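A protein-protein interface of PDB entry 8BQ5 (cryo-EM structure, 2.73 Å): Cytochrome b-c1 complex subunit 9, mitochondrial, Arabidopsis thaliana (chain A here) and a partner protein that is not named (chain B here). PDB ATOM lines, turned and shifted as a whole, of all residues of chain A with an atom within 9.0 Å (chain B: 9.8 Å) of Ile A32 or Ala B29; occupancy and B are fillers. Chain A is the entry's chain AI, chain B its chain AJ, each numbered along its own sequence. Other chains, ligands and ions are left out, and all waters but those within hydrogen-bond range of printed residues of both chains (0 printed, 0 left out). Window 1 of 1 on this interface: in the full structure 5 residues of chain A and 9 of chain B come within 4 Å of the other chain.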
ATOM      1  N   ASN A  24       1.928 -20.947  14.236  1.00  0.00           N
ATOM      2  CA  ASN A  24       3.159 -21.134  14.992  1.00  0.00           C
ATOM      3  C   ASN A  24       3.409 -19.984  15.958  1.00  0.00           C
ATOM      4  O   ASN A  24       4.071 -20.173  16.984  1.00  0.00           O
ATOM      5  CB  ASN A  24       4.345 -21.300  14.045  1.00  0.00           C
ATOM      6  CG  ASN A  24       5.529 -21.963  14.713  1.00  0.00           C
ATOM      7  OD1 ASN A  24       5.384 -22.985  15.382  1.00  0.00           O
ATOM      8  ND2 ASN A  24       6.709 -21.382  14.538  1.00  0.00           N
ATOM      9  N   SER A  25       2.902 -18.789  15.647  1.00  0.00           N
ATOM     10  CA  SER A  25       3.047 -17.664  16.563  1.00  0.00           C
ATOM     11  C   SER A  25       2.296 -17.921  17.863  1.00  0.00           C
ATOM     12  O   SER A  25       2.785 -17.604  18.953  1.00  0.00           O
ATOM     13  CB  SER A  25       2.555 -16.379  15.899  1.00  0.00           C
ATOM     14  OG  SER A  25       1.420 -16.630  15.089  1.00  0.00           O
ATOM     15  N   VAL A  26       1.094 -18.491  17.764  1.00  0.00           N
ATOM     16  CA  VAL A  26       0.337 -18.849  18.960  1.00  0.00           C
ATOM     17  C   VAL A  26       0.993 -20.025  19.671  1.00  0.00           C
ATOM     18  O   VAL A  26       1.053 -20.069  20.906  1.00  0.00           O
ATOM     19  CB  VAL A  26      -1.127 -19.149  18.592  1.00  0.00           C
ATOM     20  CG1 VAL A  26      -1.923 -19.515  19.832  1.00  0.00           C
ATOM     21  CG2 VAL A  26      -1.747 -17.956  17.890  1.00  0.00           C
ATOM     22  N   TYR A  27       1.491 -20.998  18.904  1.00  0.00           N
ATOM     23  CA  TYR A  27       2.143 -22.160  19.502  1.00  0.00           C
ATOM     24  C   TYR A  27       3.402 -21.758  20.260  1.00  0.00           C
ATOM     25  O   TYR A  27       3.673 -22.279  21.348  1.00  0.00           O
ATOM     26  CB  TYR A  27       2.474 -23.187  18.420  1.00  0.00           C
ATOM     27  CG  TYR A  27       3.002 -24.498  18.953  1.00  0.00           C
ATOM     28  CD1 TYR A  27       2.269 -25.247  19.862  1.00  0.00           C
ATOM     29  CD2 TYR A  27       4.239 -24.983  18.552  1.00  0.00           C
ATOM     30  CE1 TYR A  27       2.749 -26.446  20.351  1.00  0.00           C
ATOM     31  CE2 TYR A  27       4.727 -26.180  19.036  1.00  0.00           C
ATOM     32  CZ  TYR A  27       3.979 -26.906  19.935  1.00  0.00           C
ATOM     33  OH  TYR A  27       4.465 -28.098  20.418  1.00  0.00           O
ATOM     34  N   VAL A  28       4.188 -20.840  19.696  1.00  0.00           N
ATOM     35  CA  VAL A  28       5.393 -20.370  20.372  1.00  0.00           C
ATOM     36  C   VAL A  28       5.030 -19.631  21.655  1.00  0.00           C
ATOM     37  O   VAL A  28       5.678 -19.805  22.694  1.00  0.00           O
ATOM     38  CB  VAL A  28       6.225 -19.493  19.418  1.00  0.00           C
ATOM     39  CG1 VAL A  28       7.110 -18.532  20.197  1.00  0.00           C
ATOM     40  CG2 VAL A  28       7.059 -20.365  18.493  1.00  0.00           C
ATOM     41  N   THR A  29       3.984 -18.802  21.606  1.00  0.00           N
ATOM     42  CA  THR A  29       3.526 -18.105  22.804  1.00  0.00           C
ATOM     43  C   THR A  29       3.017 -19.088  23.852  1.00  0.00           C
ATOM     44  O   THR A  29       3.209 -18.880  25.055  1.00  0.00           O
ATOM     45  CB  THR A  29       2.439 -17.096  22.435  1.00  0.00           C
ATOM     46  OG1 THR A  29       2.894 -16.281  21.348  1.00  0.00           O
ATOM     47  CG2 THR A  29       2.107 -16.204  23.620  1.00  0.00           C
ATOM     48  N   PHE A  30       2.358 -20.162  23.411  1.00  0.00           N
ATOM     49  CA  PHE A  30       1.900 -21.193  24.339  1.00  0.00           C
ATOM     50  C   PHE A  30       3.076 -21.868  25.034  1.00  0.00           C
ATOM     51  O   PHE A  30       3.019 -22.146  26.238  1.00  0.00           O
ATOM     52  CB  PHE A  30       1.043 -22.214  23.588  1.00  0.00           C
ATOM     53  CG  PHE A  30       0.783 -23.484  24.350  1.00  0.00           C
ATOM     54  CD1 PHE A  30      -0.057 -23.492  25.450  1.00  0.00           C
ATOM     55  CD2 PHE A  30       1.358 -24.679  23.946  1.00  0.00           C
ATOM     56  CE1 PHE A  30      -0.303 -24.662  26.144  1.00  0.00           C
ATOM     57  CE2 PHE A  30       1.115 -25.852  24.635  1.00  0.00           C
ATOM     58  CZ  PHE A  30       0.284 -25.842  25.735  1.00  0.00           C
ATOM     59  N   ILE A  31       4.152 -22.139  24.292  1.00  0.00           N
ATOM     60  CA  ILE A  31       5.337 -22.750  24.889  1.00  0.00           C
ATOM     61  C   ILE A  31       5.980 -21.803  25.893  1.00  0.00           C
ATOM     62  O   ILE A  31       6.432 -22.225  26.967  1.00  0.00           O
ATOM     63  CB  ILE A  31       6.327 -23.179  23.788  1.00  0.00           C
ATOM     64  CG1 ILE A  31       5.812 -24.430  23.074  1.00  0.00           C
ATOM     65  CG2 ILE A  31       7.708 -23.435  24.368  1.00  0.00           C
ATOM     66  CD1 ILE A  31       6.504 -24.708  21.763  1.00  0.00           C
ATOM     67  N   ILE A  32       6.032 -20.511  25.567  1.00  0.00           N
ATOM     68  CA  ILE A  32       6.624 -19.532  26.476  1.00  0.00           C
ATOM     69  C   ILE A  32       5.828 -19.465  27.774  1.00  0.00           C
ATOM     70  O   ILE A  32       6.395 -19.430  28.873  1.00  0.00           O
ATOM     71  CB  ILE A  32       6.718 -18.156  25.793  1.00  0.00           C
ATOM     72  CG1 ILE A  32       7.954 -18.091  24.898  1.00  0.00           C
ATOM     73  CG2 ILE A  32       6.771 -17.042  26.826  1.00  0.00           C
ATOM     74  CD1 ILE A  32       7.845 -17.072  23.789  1.00  0.00           C
ATOM     75  N   ALA A  33       4.497 -19.453  27.666  1.00  0.00           N
ATOM     76  CA  ALA A  33       3.658 -19.425  28.860  1.00  0.00           C
ATOM     77  C   ALA A  33       3.787 -20.717  29.659  1.00  0.00           C
ATOM     78  O   ALA A  33       3.771 -20.695  30.895  1.00  0.00           O
ATOM     79  CB  ALA A  33       2.201 -19.175  28.474  1.00  0.00           C
ATOM     80  N   GLY A  34       3.899 -21.854  28.970  1.00  0.00           N
ATOM     81  CA  GLY A  34       4.042 -23.120  29.670  1.00  0.00           C
ATOM     82  C   GLY A  34       5.347 -23.221  30.434  1.00  0.00           C
ATOM     83  O   GLY A  34       5.391 -23.764  31.539  1.00  0.00           O
ATOM     84  N   ALA A  35       6.433 -22.714  29.847  1.00  0.00           N
ATOM     85  CA  ALA A  35       7.708 -22.674  30.554  1.00  0.00           C
ATOM     86  C   ALA A  35       7.636 -21.738  31.753  1.00  0.00           C
ATOM     87  O   ALA A  35       8.172 -22.040  32.825  1.00  0.00           O
ATOM     88  CB  ALA A  35       8.824 -22.249  29.600  1.00  0.00           C
ATOM     89  N   PHE A  36       6.976 -20.592  31.588  1.00  0.00           N
ATOM     90  CA  PHE A  36       6.853 -19.633  32.680  1.00  0.00           C
ATOM     91  C   PHE A  36       6.033 -20.210  33.828  1.00  0.00           C
ATOM     92  O   PHE A  36       6.504 -20.295  34.968  1.00  0.00           O
ATOM     93  CB  PHE A  36       6.222 -18.339  32.167  1.00  0.00           C
ATOM     94  CG  PHE A  36       5.968 -17.325  33.240  1.00  0.00           C
ATOM     95  CD1 PHE A  36       6.995 -16.534  33.720  1.00  0.00           C
ATOM     96  CD2 PHE A  36       4.701 -17.172  33.778  1.00  0.00           C
ATOM     97  CE1 PHE A  36       6.763 -15.605  34.711  1.00  0.00           C
ATOM     98  CE2 PHE A  36       4.463 -16.245  34.771  1.00  0.00           C
ATOM     99  CZ  PHE A  36       5.495 -15.462  35.237  1.00  0.00           C
ATOM    100  N   PHE A  37       4.796 -20.615  33.540  1.00  0.00           N
ATOM    101  CA  PHE A  37       3.917 -21.121  34.588  1.00  0.00           C
ATOM    102  C   PHE A  37       4.376 -22.481  35.097  1.00  0.00           C
ATOM    103  O   PHE A  37       4.261 -22.771  36.293  1.00  0.00           O
ATOM    104  CB  PHE A  37       2.483 -21.196  34.068  1.00  0.00           C
ATOM    105  CG  PHE A  37       1.816 -19.860  33.942  1.00  0.00           C
ATOM    106  CD1 PHE A  37       1.693 -19.029  35.042  1.00  0.00           C
ATOM    107  CD2 PHE A  37       1.325 -19.428  32.722  1.00  0.00           C
ATOM    108  CE1 PHE A  37       1.082 -17.796  34.931  1.00  0.00           C
ATOM    109  CE2 PHE A  37       0.715 -18.195  32.604  1.00  0.00           C
ATOM    110  CZ  PHE A  37       0.592 -17.377  33.710  1.00  0.00           C
ATOM    111  N   GLY A  38       4.888 -23.331  34.205  1.00  0.00           N
ATOM    112  CA  GLY A  38       5.323 -24.651  34.626  1.00  0.00           C
ATOM    113  C   GLY A  38       6.501 -24.605  35.580  1.00  0.00           C
ATOM    114  O   GLY A  38       6.545 -25.348  36.564  1.00  0.00           O
ATOM    115  N   GLU A  39       7.472 -23.731  35.305  1.00  0.00           N
ATOM    116  CA  GLU A  39       8.618 -23.597  36.195  1.00  0.00           C
ATOM    117  C   GLU A  39       8.201 -23.029  37.546  1.00  0.00           C
ATOM    118  O   GLU A  39       8.718 -23.446  38.589  1.00  0.00           O
ATOM    119  CB  GLU A  39       9.685 -22.721  35.539  1.00  0.00           C
ATOM    120  CG  GLU A  39      11.075 -22.878  36.126  1.00  0.00           C
ATOM    121  CD  GLU A  39      11.718 -21.547  36.454  1.00  0.00           C
ATOM    122  OE1 GLU A  39      12.916 -21.534  36.806  1.00  0.00           O
ATOM    123  OE2 GLU A  39      11.024 -20.511  36.358  1.00  0.00           O
ATOM    124  N   GLN B  21      -1.677  -9.983  10.494  1.00  0.00           N
ATOM    125  CA  GLN B  21      -1.966 -10.884  11.605  1.00  0.00           C
ATOM    126  C   GLN B  21      -0.723 -11.659  12.021  1.00  0.00           C
ATOM    127  O   GLN B  21      -0.539 -11.964  13.206  1.00  0.00           O
ATOM    128  CB  GLN B  21      -3.097 -11.841  11.232  1.00  0.00           C
ATOM    129  CG  GLN B  21      -4.013 -11.315  10.146  1.00  0.00           C
ATOM    130  CD  GLN B  21      -5.335 -12.050  10.092  1.00  0.00           C
ATOM    131  OE1 GLN B  21      -5.722 -12.727  11.045  1.00  0.00           O
ATOM    132  NE2 GLN B  21      -6.038 -11.920   8.974  1.00  0.00           N
ATOM    133  N   ALA B  22       0.137 -11.998  11.058  1.00  0.00           N
ATOM    134  CA  ALA B  22       1.402 -12.641  11.394  1.00  0.00           C
ATOM    135  C   ALA B  22       2.279 -11.721  12.232  1.00  0.00           C
ATOM    136  O   ALA B  22       2.928 -12.167  13.185  1.00  0.00           O
ATOM    137  CB  ALA B  22       2.131 -13.067  10.120  1.00  0.00           C
ATOM    138  N   ALA B  23       2.318 -10.432  11.885  1.00  0.00           N
ATOM    139  CA  ALA B  23       3.103  -9.479  12.664  1.00  0.00           C
ATOM    140  C   ALA B  23       2.536  -9.309  14.068  1.00  0.00           C
ATOM    141  O   ALA B  23       3.288  -9.276  15.049  1.00  0.00           O
ATOM    142  CB  ALA B  23       3.161  -8.132  11.943  1.00  0.00           C
ATOM    143  N   ALA B  24       1.211  -9.196  14.183  1.00  0.00           N
ATOM    144  CA  ALA B  24       0.593  -9.053  15.497  1.00  0.00           C
ATOM    145  C   ALA B  24       0.788 -10.310  16.337  1.00  0.00           C
ATOM    146  O   ALA B  24       1.026 -10.225  17.548  1.00  0.00           O
ATOM    147  CB  ALA B  24      -0.893  -8.731  15.347  1.00  0.00           C
ATOM    148  N   GLY B  25       0.686 -11.485  15.714  1.00  0.00           N
ATOM    149  CA  GLY B  25       0.905 -12.720  16.449  1.00  0.00           C
ATOM    150  C   GLY B  25       2.331 -12.851  16.947  1.00  0.00           C
ATOM    151  O   GLY B  25       2.572 -13.270  18.082  1.00  0.00           O
ATOM    152  N   TRP B  26       3.299 -12.494  16.101  1.00  0.00           N
ATOM    153  CA  TRP B  26       4.697 -12.565  16.513  1.00  0.00           C
ATOM    154  C   TRP B  26       5.046 -11.463  17.506  1.00  0.00           C
ATOM    155  O   TRP B  26       5.952 -11.639  18.328  1.00  0.00           O
ATOM    156  CB  TRP B  26       5.610 -12.496  15.291  1.00  0.00           C
ATOM    157  CG  TRP B  26       5.725 -13.798  14.552  1.00  0.00           C
ATOM    158  CD1 TRP B  26       5.428 -14.023  13.240  1.00  0.00           C
ATOM    159  CD2 TRP B  26       6.174 -15.053  15.082  1.00  0.00           C
ATOM    160  NE1 TRP B  26       5.659 -15.338  12.920  1.00  0.00           N
ATOM    161  CE2 TRP B  26       6.119 -15.991  14.033  1.00  0.00           C
ATOM    162  CE3 TRP B  26       6.617 -15.473  16.340  1.00  0.00           C
ATOM    163  CZ2 TRP B  26       6.489 -17.324  14.203  1.00  0.00           C
ATOM    164  CZ3 TRP B  26       6.983 -16.796  16.506  1.00  0.00           C
ATOM    165  CH2 TRP B  26       6.917 -17.705  15.444  1.00  0.00           C
ATOM    166  N   GLY B  27       4.350 -10.327  17.442  1.00  0.00           N
ATOM    167  CA  GLY B  27       4.560  -9.286  18.435  1.00  0.00           C
ATOM    168  C   GLY B  27       4.131  -9.718  19.824  1.00  0.00           C
ATOM    169  O   GLY B  27       4.777  -9.377  20.818  1.00  0.00           O
ATOM    170  N   ILE B  28       3.028 -10.464  19.912  1.00  0.00           N
ATOM    171  CA  ILE B  28       2.601 -11.023  21.193  1.00  0.00           C
ATOM    172  C   ILE B  28       3.643 -12.004  21.715  1.00  0.00           C
ATOM    173  O   ILE B  28       3.968 -12.012  22.908  1.00  0.00           O
ATOM    174  CB  ILE B  28       1.211 -11.676  21.055  1.00  0.00           C
ATOM    175  CG1 ILE B  28       0.102 -10.683  21.424  1.00  0.00           C
ATOM    176  CG2 ILE B  28       1.103 -12.929  21.913  1.00  0.00           C
ATOM    177  CD1 ILE B  28       0.034  -9.455  20.541  1.00  0.00           C
ATOM    178  N   ALA B  29       4.185 -12.844  20.829  1.00  0.00           N
ATOM    179  CA  ALA B  29       5.227 -13.782  21.236  1.00  0.00           C
ATOM    180  C   ALA B  29       6.473 -13.049  21.717  1.00  0.00           C
ATOM    181  O   ALA B  29       7.086 -13.440  22.718  1.00  0.00           O
ATOM    182  CB  ALA B  29       5.572 -14.722  20.082  1.00  0.00           C
ATOM    183  N   ALA B  30       6.869 -11.987  21.012  1.00  0.00           N
ATOM    184  CA  ALA B  30       8.026 -11.207  21.439  1.00  0.00           C
ATOM    185  C   ALA B  30       7.770 -10.544  22.787  1.00  0.00           C
ATOM    186  O   ALA B  30       8.659 -10.501  23.644  1.00  0.00           O
ATOM    187  CB  ALA B  30       8.379 -10.163  20.381  1.00  0.00           C
ATOM    188  N   ALA B  31       6.563 -10.013  22.987  1.00  0.00           N
ATOM    189  CA  ALA B  31       6.208  -9.451  24.285  1.00  0.00           C
ATOM    190  C   ALA B  31       6.170 -10.532  25.358  1.00  0.00           C
ATOM    191  O   ALA B  31       6.677 -10.338  26.468  1.00  0.00           O
ATOM    192  CB  ALA B  31       4.862  -8.731  24.196  1.00  0.00           C
ATOM    193  N   ALA B  32       5.576 -11.685  25.039  1.00  0.00           N
ATOM    194  CA  ALA B  32       5.495 -12.769  26.014  1.00  0.00           C
ATOM    195  C   ALA B  32       6.880 -13.275  26.393  1.00  0.00           C
ATOM    196  O   ALA B  32       7.147 -13.558  27.566  1.00  0.00           O
ATOM    197  CB  ALA B  32       4.638 -13.910  25.465  1.00  0.00           C
ATOM    198  N   GLY B  33       7.773 -13.403  25.411  1.00  0.00           N
ATOM    199  CA  GLY B  33       9.129 -13.827  25.712  1.00  0.00           C
ATOM    200  C   GLY B  33       9.891 -12.805  26.532  1.00  0.00           C
ATOM    201  O   GLY B  33      10.663 -13.163  27.424  1.00  0.00           O
ATOM    202  N   ALA B  34       9.686 -11.518  26.239  1.00  0.00           N
ATOM    203  CA  ALA B  34      10.382 -10.466  26.973  1.00  0.00           C
ATOM    204  C   ALA B  34       9.998 -10.476  28.448  1.00  0.00           C
ATOM    205  O   ALA B  34      10.856 -10.340  29.326  1.00  0.00           O
ATOM    206  CB  ALA B  34      10.083  -9.104  26.346  1.00  0.00           C
ATOM    207  N   ILE B  35       8.705 -10.641  28.739  1.00  0.00           N
ATOM    208  CA  ILE B  35       8.261 -10.729  30.128  1.00  0.00           C
ATOM    209  C   ILE B  35       8.710 -12.044  30.749  1.00  0.00           C
ATOM    210  O   ILE B  35       8.706 -12.198  31.977  1.00  0.00           O
ATOM    211  CB  ILE B  35       6.730 -10.553  30.212  1.00  0.00           C
ATOM    212  CG1 ILE B  35       6.286  -9.346  29.387  1.00  0.00           C
ATOM    213  CG2 ILE B  35       6.279 -10.365  31.652  1.00  0.00           C
ATOM    214  CD1 ILE B  35       4.791  -9.283  29.163  1.00  0.00           C
ATOM    215  N   TRP B  36       9.118 -13.005  29.921  1.00  0.00           N
ATOM    216  CA  TRP B  36       9.522 -14.305  30.440  1.00  0.00           C
ATOM    217  C   TRP B  36      11.007 -14.341  30.783  1.00  0.00           C
ATOM    218  O   TRP B  36      11.388 -14.862  31.837  1.00  0.00           O
ATOM    219  CB  TRP B  36       9.172 -15.393  29.425  1.00  0.00           C
ATOM    220  CG  TRP B  36       9.831 -16.701  29.692  1.00  0.00           C
ATOM    221  CD1 TRP B  36       9.683 -17.487  30.795  1.00  0.00           C
ATOM    222  CD2 TRP B  36      10.751 -17.380  28.835  1.00  0.00           C
ATOM    223  NE1 TRP B  36      10.452 -18.617  30.677  1.00  0.00           N
ATOM    224  CE2 TRP B  36      11.119 -18.575  29.481  1.00  0.00           C
ATOM    225  CE3 TRP B  36      11.300 -17.095  27.582  1.00  0.00           C
ATOM    226  CZ2 TRP B  36      12.009 -19.483  28.918  1.00  0.00           C
ATOM    227  CZ3 TRP B  36      12.183 -17.996  27.024  1.00  0.00           C
ATOM    228  CH2 TRP B  36      12.530 -19.175  27.692  1.00  0.00           C
ATOM    229  N   VAL B  37      11.861 -13.795  29.916  1.00  0.00           N
ATOM    230  CA  VAL B  37      13.296 -13.756  30.180  1.00  0.00           C
ATOM    231  C   VAL B  37      13.554 -12.764  31.306  1.00  0.00           C
ATOM    232  O   VAL B  37      14.075 -13.127  32.366  1.00  0.00           O
ATOM    233  CB  VAL B  37      14.096 -13.382  28.921  1.00  0.00           C
ATOM    234  CG1 VAL B  37      15.585 -13.535  29.181  1.00  0.00           C
ATOM    235  CG2 VAL B  37      13.671 -14.245  27.747  1.00  0.00           C
ATOM    236  N   VAL B  38      13.195 -11.508  31.077  1.00  0.00           N
ATOM    237  CA  VAL B  38      13.181 -10.509  32.136  1.00  0.00           C
ATOM    238  C   VAL B  38      11.805 -10.515  32.780  1.00  0.00           C
ATOM    239  O   VAL B  38      10.787 -10.357  32.097  1.00  0.00           O
ATOM    240  CB  VAL B  38      13.529  -9.118  31.577  1.00  0.00           C
ATOM    241  CG1 VAL B  38      13.983  -8.194  32.694  1.00  0.00           C
ATOM    242  CG2 VAL B  38      14.593  -9.228  30.497  1.00  0.00           C
ATOM    243  N   GLN B  39      11.760 -10.712  34.099  1.00  0.00           N
ATOM    244  CA  GLN B  39      10.507 -10.815  34.844  1.00  0.00           C
ATOM    245  C   GLN B  39      10.405  -9.611  35.772  1.00  0.00           C
ATOM    246  O   GLN B  39      10.683  -9.716  36.977  1.00  0.00           O
ATOM    247  CB  GLN B  39      10.432 -12.132  35.614  1.00  0.00           C
ATOM    248  CG  GLN B  39      10.328 -13.356  34.716  1.00  0.00           C
ATOM    249  CD  GLN B  39      10.143 -14.645  35.491  1.00  0.00           C
ATOM    250  OE1 GLN B  39      10.024 -14.636  36.716  1.00  0.00           O
ATOM    251  NE2 GLN B  39      10.119 -15.764  34.778  1.00  0.00           N
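Asn A24 touches Trp B26.
Ser A25 touches Gly B25 (CB to C, 3.7 Å).
Ser A25 touches Trp B26.
CG2 of Thr A29 touches CG2 of Ile B28, at 3.8 Å.
CG2 of Thr A29 touches CB of Ala B32 (3.9 Å).
Ala B32 touches Ile A32.
Gly B33 touches Ile A32 (CA to CD1, 3.98 Å).
Ile A32 touches Trp B36.
CD1 of Trp B36 touches CB of Phe A36, 3.8 Å away.
Phe A36 touches Gln B39.
Printed residues of chain B within 4 Å of Ile A32: Ala B29 (3.9 Å), Ala B32 (3.6 Å), Gly B33 (3.98 Å) and Trp B36 (3.9 Å).
Thr A29 touches just these residues of chain B: Ile B28, Ala B29 and Ala B32.
No residue of chain B comes within 4 Å of Ala A33.
No residue of chain B comes within 4 Å of Gly A34.
No residue of chain B comes within 4 Å of Ala A35.
Gly B27 touches none of the printed residues of chain A.
Printed residues of chain A within 4 Å of Ala B32: Thr A29 (3.9 Å) and Ile A32 (3.6 Å).
Of the printed residues of chain A, Trp B26 touches Asn A24 and Ser A25.
Of the printed residues of chain B, Asn A24 touches Trp B26 (3.8 Å).
Of the printed residues of chain B, Ser A25 touches Gly B25 (3.7 Å) and Trp B26 (3.9 Å).
The nearest printed residue of chain A that does not touch Ile B28 is Ser A25 (5.8 Å).
The backbone carbonyl oxygen (O) of Trp B36 is in hydrogen-bond range of the side-chain amide nitrogen (NE2) of Gln B39 (3.3 Å).
OG1 of Thr A29 lies within hydrogen-bond range of O of Ser A25, at 2.7 Å.
Of the 19 printed residues of chain B, 8 touch a printed residue of chain A.
Hydrophobic or aromatic side chains of chain B within 4 Å of the printed part of chain A: Trp B26, Ile B28, Ala B29, Ala B32 and Trp B36.
Printed residues of chain A that touch a printed residue of chain B: Asn A24, Ser A25, Thr A29, Ile A32 and Phe A36.
Hydrophobic or aromatic side chains of chain A that line the printed part of chain B: Ile A32 and Phe A36.
Among the printed residues, no Asp or Glu carboxylate lies within 4 Å of a Lys or Arg side-chain nitrogen of the other chain.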
